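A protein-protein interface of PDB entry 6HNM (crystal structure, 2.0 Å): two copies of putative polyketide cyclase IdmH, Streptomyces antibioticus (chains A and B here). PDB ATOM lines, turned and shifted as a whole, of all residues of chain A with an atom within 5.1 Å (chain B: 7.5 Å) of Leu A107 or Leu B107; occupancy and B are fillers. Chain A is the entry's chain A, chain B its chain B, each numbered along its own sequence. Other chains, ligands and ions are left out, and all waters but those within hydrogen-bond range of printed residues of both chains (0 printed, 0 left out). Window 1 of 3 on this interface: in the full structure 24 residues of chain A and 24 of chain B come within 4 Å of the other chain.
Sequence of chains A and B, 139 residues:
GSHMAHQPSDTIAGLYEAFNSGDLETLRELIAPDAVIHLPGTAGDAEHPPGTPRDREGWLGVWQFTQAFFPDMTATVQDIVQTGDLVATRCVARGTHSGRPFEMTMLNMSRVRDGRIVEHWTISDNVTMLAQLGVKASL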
ATOM      1  N   THR A  89       2.985 -27.613  21.850  1.00  0.00           N
ATOM      2  CA  THR A  89       3.310 -28.597  22.880  1.00  0.00           C
ATOM      3  C   THR A  89       2.315 -28.561  24.027  1.00  0.00           C
ATOM      4  O   THR A  89       1.833 -27.476  24.417  1.00  0.00           O
ATOM      5  CB  THR A  89       4.714 -28.380  23.474  1.00  0.00           C
ATOM      6  OG1 THR A  89       4.920 -26.995  23.782  1.00  0.00           O
ATOM      7  CG2 THR A  89       5.779 -28.843  22.490  1.00  0.00           C
ATOM      8  N   ARG A  90       2.014 -29.746  24.563  1.00  0.00           N
ATOM      9  CA  ARG A  90       1.383 -29.870  25.865  1.00  0.00           C
ATOM     10  C   ARG A  90       2.446 -30.360  26.823  1.00  0.00           C
ATOM     11  O   ARG A  90       3.087 -31.392  26.569  1.00  0.00           O
ATOM     12  CB  ARG A  90       0.215 -30.850  25.843  1.00  0.00           C
ATOM     13  CG  ARG A  90      -0.439 -31.037  27.200  1.00  0.00           C
ATOM     14  CD  ARG A  90      -1.667 -31.923  27.116  1.00  0.00           C
ATOM     15  NE  ARG A  90      -1.360 -33.289  26.689  1.00  0.00           N
ATOM     16  CZ  ARG A  90      -0.937 -34.278  27.483  1.00  0.00           C
ATOM     17  NH1 ARG A  90      -0.722 -34.090  28.785  1.00  0.00           N
ATOM     18  NH2 ARG A  90      -0.727 -35.486  26.953  1.00  0.00           N
ATOM     19  N   CYS A  91       2.639 -29.617  27.910  1.00  0.00           N
ATOM     20  CA  CYS A  91       3.586 -29.998  28.942  1.00  0.00           C
ATOM     21  C   CYS A  91       2.862 -30.191  30.251  1.00  0.00           C
ATOM     22  O   CYS A  91       1.751 -29.664  30.446  1.00  0.00           O
ATOM     23  CB  CYS A  91       4.654 -28.925  29.150  1.00  0.00           C
ATOM     24  SG  CYS A  91       5.584 -28.441  27.697  1.00  0.00           S
ATOM     25  N   THR A 105      -1.091 -28.567  33.873  1.00  0.00           N
ATOM     26  CA  THR A 105      -0.981 -28.535  32.420  1.00  0.00           C
ATOM     27  C   THR A 105      -0.480 -27.174  31.925  1.00  0.00           C
ATOM     28  O   THR A 105      -0.868 -26.116  32.456  1.00  0.00           O
ATOM     29  CB  THR A 105      -2.332 -28.847  31.763  1.00  0.00           C
ATOM     30  OG1 THR A 105      -2.806 -30.112  32.240  1.00  0.00           O
ATOM     31  CG2 THR A 105      -2.212 -28.891  30.231  1.00  0.00           C
ATOM     32  N   MET A 106       0.418 -27.216  30.937  1.00  0.00           N
ATOM     33  CA  MET A 106       0.828 -26.039  30.168  1.00  0.00           C
ATOM     34  C   MET A 106       0.576 -26.324  28.695  1.00  0.00           C
ATOM     35  O   MET A 106       0.896 -27.421  28.203  1.00  0.00           O
ATOM     36  CB  MET A 106       2.316 -25.758  30.300  1.00  0.00           C
ATOM     37  CG  MET A 106       2.887 -25.671  31.702  1.00  0.00           C
ATOM     38  SD  MET A 106       4.691 -25.596  31.655  1.00  0.00           S
ATOM     39  CE  MET A 106       4.976 -24.291  30.434  1.00  0.00           C
ATOM     40  N   LEU A 107       0.026 -25.346  27.978  1.00  0.00           N
ATOM     41  CA  LEU A 107      -0.105 -25.429  26.542  1.00  0.00           C
ATOM     42  C   LEU A 107       0.711 -24.299  25.946  1.00  0.00           C
ATOM     43  O   LEU A 107       0.665 -23.153  26.434  1.00  0.00           O
ATOM     44  CB  LEU A 107      -1.564 -25.315  26.128  1.00  0.00           C
ATOM     45  CG  LEU A 107      -2.450 -26.467  26.591  1.00  0.00           C
ATOM     46  CD1 LEU A 107      -3.879 -26.178  26.175  1.00  0.00           C
ATOM     47  CD2 LEU A 107      -1.995 -27.807  26.017  1.00  0.00           C
ATOM     48  N   ASN A 108       1.461 -24.626  24.896  1.00  0.00           N
ATOM     49  CA  ASN A 108       2.362 -23.682  24.255  1.00  0.00           C
ATOM     50  C   ASN A 108       2.285 -23.823  22.751  1.00  0.00           C
ATOM     51  O   ASN A 108       2.004 -24.902  22.238  1.00  0.00           O
ATOM     52  CB  ASN A 108       3.811 -23.929  24.666  1.00  0.00           C
ATOM     53  CG  ASN A 108       3.951 -24.301  26.120  1.00  0.00           C
ATOM     54  OD1 ASN A 108       3.822 -23.451  27.000  1.00  0.00           O
ATOM     55  ND2 ASN A 108       4.237 -25.574  26.381  1.00  0.00           N
ATOM     56  N   MET A 109       2.579 -22.734  22.062  1.00  0.00           N
ATOM     57  CA  MET A 109       2.667 -22.724  20.612  1.00  0.00           C
ATOM     58  C   MET A 109       3.834 -21.828  20.259  1.00  0.00           C
ATOM     59  O   MET A 109       3.941 -20.722  20.777  1.00  0.00           O
ATOM     60  CB  MET A 109       1.368 -22.211  19.999  1.00  0.00           C
ATOM     61  CG  MET A 109       1.390 -22.151  18.487  1.00  0.00           C
ATOM     62  SD  MET A 109      -0.218 -22.236  17.680  1.00  0.00           S
ATOM     63  CE  MET A 109      -1.058 -23.630  18.455  1.00  0.00           C
ATOM     64  N   TRP A 121       3.514 -18.476  22.275  1.00  0.00           N
ATOM     65  CA  TRP A 121       2.335 -18.285  23.095  1.00  0.00           C
ATOM     66  C   TRP A 121       2.352 -19.378  24.149  1.00  0.00           C
ATOM     67  O   TRP A 121       2.631 -20.546  23.818  1.00  0.00           O
ATOM     68  CB  TRP A 121       1.066 -18.435  22.265  1.00  0.00           C
ATOM     69  CG  TRP A 121       0.866 -17.429  21.166  1.00  0.00           C
ATOM     70  CD1 TRP A 121       0.099 -16.289  21.225  1.00  0.00           C
ATOM     71  CD2 TRP A 121       1.384 -17.490  19.832  1.00  0.00           C
ATOM     72  NE1 TRP A 121       0.126 -15.639  20.017  1.00  0.00           N
ATOM     73  CE2 TRP A 121       0.902 -16.356  19.143  1.00  0.00           C
ATOM     74  CE3 TRP A 121       2.207 -18.395  19.151  1.00  0.00           C
ATOM     75  CZ2 TRP A 121       1.229 -16.091  17.808  1.00  0.00           C
ATOM     76  CZ3 TRP A 121       2.534 -18.133  17.807  1.00  0.00           C
ATOM     77  CH2 TRP A 121       2.045 -16.986  17.156  1.00  0.00           C
ATOM     78  N   THR A 122       2.057 -19.019  25.399  1.00  0.00           N
ATOM     79  CA  THR A 122       1.969 -20.011  26.482  1.00  0.00           C
ATOM     80  C   THR A 122       0.902 -19.614  27.504  1.00  0.00           C
ATOM     81  O   THR A 122       0.685 -18.422  27.765  1.00  0.00           O
ATOM     82  CB  THR A 122       3.332 -20.253  27.172  1.00  0.00           C
ATOM     83  OG1 THR A 122       3.226 -21.317  28.143  1.00  0.00           O
ATOM     84  CG2 THR A 122       3.848 -18.994  27.848  1.00  0.00           C
ATOM     85  N   ILE A 123       0.203 -20.614  28.022  1.00  0.00           N
ATOM     86  CA  ILE A 123      -0.711 -20.435  29.150  1.00  0.00           C
ATOM     87  C   ILE A 123      -0.586 -21.672  30.032  1.00  0.00           C
ATOM     88  O   ILE A 123      -0.432 -22.789  29.539  1.00  0.00           O
ATOM     89  CB  ILE A 123      -2.200 -20.277  28.743  1.00  0.00           C
ATOM     90  CG1 ILE A 123      -2.387 -19.258  27.614  1.00  0.00           C
ATOM     91  CG2 ILE A 123      -3.023 -19.828  29.944  1.00  0.00           C
ATOM     92  CD1 ILE A 123      -3.816 -19.152  27.111  1.00  0.00           C
ATOM     93  N   TYR B  16     -15.324 -25.436  16.642  1.00  0.00           N
ATOM     94  CA  TYR B  16     -15.393 -24.039  17.068  1.00  0.00           C
ATOM     95  C   TYR B  16     -16.504 -23.276  16.337  1.00  0.00           C
ATOM     96  O   TYR B  16     -17.186 -22.453  16.952  1.00  0.00           O
ATOM     97  CB  TYR B  16     -14.015 -23.361  17.006  1.00  0.00           C
ATOM     98  CG  TYR B  16     -13.136 -23.903  18.122  1.00  0.00           C
ATOM     99  CD1 TYR B  16     -13.453 -23.655  19.458  1.00  0.00           C
ATOM    100  CD2 TYR B  16     -12.043 -24.729  17.853  1.00  0.00           C
ATOM    101  CE1 TYR B  16     -12.690 -24.177  20.487  1.00  0.00           C
ATOM    102  CE2 TYR B  16     -11.279 -25.264  18.886  1.00  0.00           C
ATOM    103  CZ  TYR B  16     -11.600 -24.985  20.192  1.00  0.00           C
ATOM    104  OH  TYR B  16     -10.846 -25.505  21.217  1.00  0.00           O
ATOM    105  N   HIS B  38     -10.218 -32.164  29.490  1.00  0.00           N
ATOM    106  CA  HIS B  38      -9.416 -31.540  30.529  1.00  0.00           C
ATOM    107  C   HIS B  38      -9.631 -30.027  30.493  1.00  0.00           C
ATOM    108  O   HIS B  38      -9.067 -29.325  29.644  1.00  0.00           O
ATOM    109  CB  HIS B  38      -7.946 -31.880  30.327  1.00  0.00           C
ATOM    110  CG  HIS B  38      -7.665 -33.353  30.258  1.00  0.00           C
ATOM    111  ND1 HIS B  38      -7.560 -34.146  31.382  1.00  0.00           N
ATOM    112  CD2 HIS B  38      -7.468 -34.172  29.195  1.00  0.00           C
ATOM    113  CE1 HIS B  38      -7.291 -35.387  31.009  1.00  0.00           C
ATOM    114  NE2 HIS B  38      -7.226 -35.428  29.690  1.00  0.00           N
ATOM    115  N   ASP B  79      -4.346 -20.169  14.493  1.00  0.00           N
ATOM    116  CA  ASP B  79      -3.337 -21.128  14.059  1.00  0.00           C
ATOM    117  C   ASP B  79      -3.817 -22.547  14.374  1.00  0.00           C
ATOM    118  O   ASP B  79      -4.487 -22.786  15.382  1.00  0.00           O
ATOM    119  CB  ASP B  79      -2.000 -20.882  14.789  1.00  0.00           C
ATOM    120  CG  ASP B  79      -1.123 -19.839  14.099  1.00  0.00           C
ATOM    121  OD1 ASP B  79      -1.010 -19.831  12.854  1.00  0.00           O
ATOM    122  OD2 ASP B  79      -0.534 -19.025  14.822  1.00  0.00           O
ATOM    123  N   ALA B  88      -3.490 -29.248  17.499  1.00  0.00           N
ATOM    124  CA  ALA B  88      -3.380 -28.141  18.439  1.00  0.00           C
ATOM    125  C   ALA B  88      -3.860 -26.889  17.738  1.00  0.00           C
ATOM    126  O   ALA B  88      -3.637 -26.717  16.532  1.00  0.00           O
ATOM    127  CB  ALA B  88      -1.959 -27.974  18.933  1.00  0.00           C
ATOM    128  N   THR B  89      -4.548 -26.034  18.491  1.00  0.00           N
ATOM    129  CA  THR B  89      -5.101 -24.785  17.955  1.00  0.00           C
ATOM    130  C   THR B  89      -4.856 -23.625  18.896  1.00  0.00           C
ATOM    131  O   THR B  89      -4.878 -23.790  20.116  1.00  0.00           O
ATOM    132  CB  THR B  89      -6.620 -24.873  17.693  1.00  0.00           C
ATOM    133  OG1 THR B  89      -7.285 -25.482  18.805  1.00  0.00           O
ATOM    134  CG2 THR B  89      -6.913 -25.677  16.481  1.00  0.00           C
ATOM    135  N   ARG B  90      -4.593 -22.459  18.309  1.00  0.00           N
ATOM    136  CA  ARG B  90      -4.661 -21.192  19.009  1.00  0.00           C
ATOM    137  C   ARG B  90      -5.892 -20.478  18.488  1.00  0.00           C
ATOM    138  O   ARG B  90      -6.030 -20.295  17.280  1.00  0.00           O
ATOM    139  CB  ARG B  90      -3.427 -20.331  18.749  1.00  0.00           C
ATOM    140  CG  ARG B  90      -3.490 -18.972  19.447  1.00  0.00           C
ATOM    141  CD  ARG B  90      -2.153 -18.250  19.417  1.00  0.00           C
ATOM    142  NE  ARG B  90      -1.768 -17.925  18.048  1.00  0.00           N
ATOM    143  CZ  ARG B  90      -2.142 -16.842  17.363  1.00  0.00           C
ATOM    144  NH1 ARG B  90      -2.946 -15.919  17.898  1.00  0.00           N
ATOM    145  NH2 ARG B  90      -1.729 -16.692  16.112  1.00  0.00           N
ATOM    146  N   CYS B  91      -6.785 -20.092  19.390  1.00  0.00           N
ATOM    147  CA  CYS B  91      -7.967 -19.319  19.031  1.00  0.00           C
ATOM    148  C   CYS B  91      -7.953 -18.000  19.768  1.00  0.00           C
ATOM    149  O   CYS B  91      -7.255 -17.835  20.772  1.00  0.00           O
ATOM    150  CB  CYS B  91      -9.258 -20.061  19.412  1.00  0.00           C
ATOM    151  SG  CYS B  91      -9.454 -21.698  18.677  1.00  0.00           S
ATOM    152  N   VAL B  92      -8.768 -17.071  19.285  1.00  0.00           N
ATOM    153  CA  VAL B  92      -9.042 -15.824  20.000  1.00  0.00           C
ATOM    154  C   VAL B  92     -10.531 -15.806  20.310  1.00  0.00           C
ATOM    155  O   VAL B  92     -11.364 -15.979  19.422  1.00  0.00           O
ATOM    156  CB  VAL B  92      -8.585 -14.570  19.222  1.00  0.00           C
ATOM    157  CG1 VAL B  92      -9.448 -14.313  17.983  1.00  0.00           C
ATOM    158  CG2 VAL B  92      -8.573 -13.350  20.130  1.00  0.00           C
ATOM    159  N   MET B 104      -9.310 -12.501  24.021  1.00  0.00           N
ATOM    160  CA  MET B 104      -8.599 -13.422  24.909  1.00  0.00           C
ATOM    161  C   MET B 104      -8.059 -14.626  24.136  1.00  0.00           C
ATOM    162  O   MET B 104      -8.777 -15.230  23.347  1.00  0.00           O
ATOM    163  CB  MET B 104      -9.579 -13.884  25.981  1.00  0.00           C
ATOM    164  CG  MET B 104      -9.125 -15.104  26.743  1.00  0.00           C
ATOM    165  SD  MET B 104     -10.216 -15.417  28.126  1.00  0.00           S
ATOM    166  CE  MET B 104     -11.604 -16.119  27.256  1.00  0.00           C
ATOM    167  N   THR B 105      -6.797 -14.973  24.377  1.00  0.00           N
ATOM    168  CA  THR B 105      -6.195 -16.143  23.731  1.00  0.00           C
ATOM    169  C   THR B 105      -6.708 -17.450  24.366  1.00  0.00           C
ATOM    170  O   THR B 105      -6.877 -17.530  25.575  1.00  0.00           O
ATOM    171  CB  THR B 105      -4.664 -16.082  23.815  1.00  0.00           C
ATOM    172  OG1 THR B 105      -4.226 -14.912  23.141  1.00  0.00           O
ATOM    173  CG2 THR B 105      -4.010 -17.296  23.140  1.00  0.00           C
ATOM    174  N   MET B 106      -6.973 -18.436  23.519  1.00  0.00           N
ATOM    175  CA  MET B 106      -7.247 -19.811  23.930  1.00  0.00           C
ATOM    176  C   MET B 106      -6.229 -20.720  23.251  1.00  0.00           C
ATOM    177  O   MET B 106      -5.999 -20.595  22.060  1.00  0.00           O
ATOM    178  CB  MET B 106      -8.629 -20.300  23.496  1.00  0.00           C
ATOM    179  CG  MET B 106      -9.804 -19.393  23.793  1.00  0.00           C
ATOM    180  SD  MET B 106     -11.313 -20.075  23.022  1.00  0.00           S
ATOM    181  CE  MET B 106     -11.324 -21.716  23.736  1.00  0.00           C
ATOM    182  N   LEU B 107      -5.654 -21.635  24.017  1.00  0.00           N
ATOM    183  CA  LEU B 107      -4.811 -22.686  23.463  1.00  0.00           C
ATOM    184  C   LEU B 107      -5.478 -24.004  23.765  1.00  0.00           C
ATOM    185  O   LEU B 107      -5.957 -24.217  24.882  1.00  0.00           O
ATOM    186  CB  LEU B 107      -3.415 -22.640  24.059  1.00  0.00           C
ATOM    187  CG  LEU B 107      -2.628 -21.381  23.751  1.00  0.00           C
ATOM    188  CD1 LEU B 107      -1.330 -21.432  24.524  1.00  0.00           C
ATOM    189  CD2 LEU B 107      -2.389 -21.220  22.255  1.00  0.00           C
ATOM    190  N   ASN B 108      -5.525 -24.869  22.751  1.00  0.00           N
ATOM    191  CA  ASN B 108      -6.240 -26.133  22.828  1.00  0.00           C
ATOM    192  C   ASN B 108      -5.408 -27.230  22.174  1.00  0.00           C
ATOM    193  O   ASN B 108      -4.650 -26.973  21.249  1.00  0.00           O
ATOM    194  CB  ASN B 108      -7.580 -26.061  22.104  1.00  0.00           C
ATOM    195  CG  ASN B 108      -8.280 -24.732  22.291  1.00  0.00           C
ATOM    196  OD1 ASN B 108      -8.798 -24.428  23.367  1.00  0.00           O
ATOM    197  ND2 ASN B 108      -8.309 -23.936  21.237  1.00  0.00           N
ATOM    198  N   MET B 109      -5.596 -28.451  22.656  1.00  0.00           N
ATOM    199  CA  MET B 109      -5.004 -29.640  22.063  1.00  0.00           C
ATOM    200  C   MET B 109      -6.072 -30.719  22.081  1.00  0.00           C
ATOM    201  O   MET B 109      -6.719 -30.935  23.097  1.00  0.00           O
ATOM    202  CB  MET B 109      -3.778 -30.062  22.859  1.00  0.00           C
ATOM    203  CG  MET B 109      -3.117 -31.361  22.390  1.00  0.00           C
ATOM    204  SD  MET B 109      -1.842 -31.157  21.154  1.00  0.00           S
ATOM    205  CE  MET B 109      -0.643 -30.168  22.043  1.00  0.00           C
ATOM    206  N   HIS B 120      -9.380 -33.842  24.870  1.00  0.00           N
ATOM    207  CA  HIS B 120      -9.261 -32.395  24.659  1.00  0.00           C
ATOM    208  C   HIS B 120      -8.657 -31.721  25.887  1.00  0.00           C
ATOM    209  O   HIS B 120      -9.037 -32.017  27.023  1.00  0.00           O
ATOM    210  CB  HIS B 120     -10.644 -31.808  24.358  1.00  0.00           C
ATOM    211  CG  HIS B 120     -10.632 -30.371  23.928  1.00  0.00           C
ATOM    212  ND1 HIS B 120     -10.243 -29.968  22.671  1.00  0.00           N
ATOM    213  CD2 HIS B 120     -11.031 -29.250  24.575  1.00  0.00           C
ATOM    214  CE1 HIS B 120     -10.371 -28.656  22.571  1.00  0.00           C
ATOM    215  NE2 HIS B 120     -10.850 -28.199  23.713  1.00  0.00           N
ATOM    216  N   TRP B 121      -7.688 -30.842  25.646  1.00  0.00           N
ATOM    217  CA  TRP B 121      -7.138 -29.972  26.669  1.00  0.00           C
ATOM    218  C   TRP B 121      -7.353 -28.541  26.183  1.00  0.00           C
ATOM    219  O   TRP B 121      -7.121 -28.256  25.006  1.00  0.00           O
ATOM    220  CB  TRP B 121      -5.647 -30.212  26.830  1.00  0.00           C
ATOM    221  CG  TRP B 121      -5.244 -31.582  27.322  1.00  0.00           C
ATOM    222  CD1 TRP B 121      -4.942 -31.937  28.610  1.00  0.00           C
ATOM    223  CD2 TRP B 121      -5.037 -32.755  26.527  1.00  0.00           C
ATOM    224  NE1 TRP B 121      -4.570 -33.258  28.663  1.00  0.00           N
ATOM    225  CE2 TRP B 121      -4.619 -33.784  27.398  1.00  0.00           C
ATOM    226  CE3 TRP B 121      -5.163 -33.038  25.161  1.00  0.00           C
ATOM    227  CZ2 TRP B 121      -4.340 -35.080  26.948  1.00  0.00           C
ATOM    228  CZ3 TRP B 121      -4.877 -34.331  24.706  1.00  0.00           C
ATOM    229  CH2 TRP B 121      -4.471 -35.333  25.600  1.00  0.00           C
ATOM    230  N   THR B 122      -7.775 -27.652  27.078  1.00  0.00           N
ATOM    231  CA  THR B 122      -7.931 -26.226  26.753  1.00  0.00           C
ATOM    232  C   THR B 122      -7.625 -25.348  27.964  1.00  0.00           C
ATOM    233  O   THR B 122      -7.876 -25.727  29.103  1.00  0.00           O
ATOM    234  CB  THR B 122      -9.338 -25.915  26.180  1.00  0.00           C
ATOM    235  OG1 THR B 122      -9.421 -24.544  25.766  1.00  0.00           O
ATOM    236  CG2 THR B 122     -10.432 -26.177  27.189  1.00  0.00           C
ATOM    237  N   ILE B 123      -7.026 -24.189  27.701  1.00  0.00           N
ATOM    238  CA  ILE B 123      -6.809 -23.161  28.711  1.00  0.00           C
ATOM    239  C   ILE B 123      -7.020 -21.809  28.039  1.00  0.00           C
ATOM    240  O   ILE B 123      -6.659 -21.626  26.874  1.00  0.00           O
ATOM    241  CB  ILE B 123      -5.384 -23.182  29.331  1.00  0.00           C
ATOM    242  CG1 ILE B 123      -4.952 -24.598  29.744  1.00  0.00           C
ATOM    243  CG2 ILE B 123      -5.342 -22.272  30.554  1.00  0.00           C
ATOM    244  CD1 ILE B 123      -3.537 -24.677  30.292  1.00  0.00           C
ATOM    245  N   SER B 124      -7.593 -20.874  28.787  1.00  0.00           N
ATOM    246  CA  SER B 124      -7.873 -19.546  28.302  1.00  0.00           C
ATOM    247  C   SER B 124      -7.149 -18.517  29.147  1.00  0.00           C
ATOM    248  O   SER B 124      -6.972 -18.703  30.353  1.00  0.00           O
ATOM    249  CB  SER B 124      -9.382 -19.328  28.317  1.00  0.00           C
ATOM    250  OG  SER B 124      -9.949 -20.065  27.265  1.00  0.00           O
ATOM    251  N   ASP B 125      -6.761 -17.414  28.507  1.00  0.00           N
ATOM    252  CA  ASP B 125      -6.059 -16.326  29.176  1.00  0.00           C
ATOM    253  C   ASP B 125      -7.050 -15.372  29.890  1.00  0.00           C
ATOM    254  O   ASP B 125      -7.181 -14.195  29.524  1.00  0.00           O
ATOM    255  CB  ASP B 125      -5.206 -15.579  28.153  1.00  0.00           C
ATOM    256  CG  ASP B 125      -4.224 -14.612  28.796  1.00  0.00           C
ATOM    257  OD1 ASP B 125      -4.098 -14.585  30.037  1.00  0.00           O
ATOM    258  OD2 ASP B 125      -3.565 -13.865  28.051  1.00  0.00           O
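Among the printed residues, merely in contact across the chains: Thr A89 with Met B109 (3.9 Å), Arg A90 with Met B109 (3.7 Å), Arg A90 with Trp B121 (3.4 Å), Thr A105 with Ile B123 (3.7 Å), Leu A107 with Leu B107 (3.1 Å), Met A109 with Asp B79 (3.7 Å), Met A109 with Thr B89 (3.8 Å), Met A109 with Arg B90 (3.7 Å), Trp A121 with Arg B90 (3.3 Å), Ile A123 with Thr B105 (3.8 Å), Ile A123 with Leu B107 (3.9 Å), Ile A123 with Ile B123 (3.4 Å), Ile A123 with Ser B124 (3.96 Å) and Ile A123 with Asp B125 (3.7 Å).
Arg A90 touches Met B109, and with the chains exchanged Met A109 touches Arg B90.
Thr A105 touches Ile B123, and with the chains exchanged Ile A123 touches Thr B105.
Ile A123 touches Leu B107, but with the chains exchanged Leu A107 does not touch Ile B123 (4.02 Å).
Ile B123 touches its own counterpart, Ile A123.
Positions printed for both chains: 89, 90, 91, 105, 106, 107, 108, 109, 121, 122 and 123.
Of the printed residues of chain B, Thr A105 touches Ile B123.
Printed residues of chain B within 4 Å of Leu A107: Leu B107 (3.1 Å).
Of the printed residues of chain A, Asp B79 touches Met A109.
Printed residues of chain A within 4 Å of Thr B89: Met A109 (3.8 Å).
Of chain A, only Leu A107 (3.1 Å) and Ile A123 (3.9 Å) come within 4 Å of Leu B107.
Of the printed residues of chain A, Asp B125 touches Ile A123.
The nearest printed residue of chain B that does not touch Thr A105 is Trp B121 (4.4 Å).
The backbone NH (N) of Trp B121 sits at hydrogen-bond distance from the backbone carbonyl oxygen (O) of Met B109 (2.7 Å).
N of Trp A121 sits at hydrogen-bond distance from O of Met A109 (2.7 Å).
The backbone carbonyl oxygen of Thr B105 sits at hydrogen-bond distance from the backbone NH of Asp B125 (2.9 Å).
O of Asn A108 sits at hydrogen-bond distance from N of Thr A89, 2.9 Å away.
The backbone NH (N) of Thr B89 is in hydrogen-bond range of the backbone carbonyl oxygen (O) of Asn B108, 2.9 Å away.
O of Ile A123 lies within hydrogen-bond range of N of Leu A107, at 3.0 Å.
Of the 20 printed residues of chain B, 10 touch a printed residue of chain A.
Among the printed residues, no Asp or Glu carboxylate lies within 4 Å of a Lys or Arg side-chain nitrogen of the other chain.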
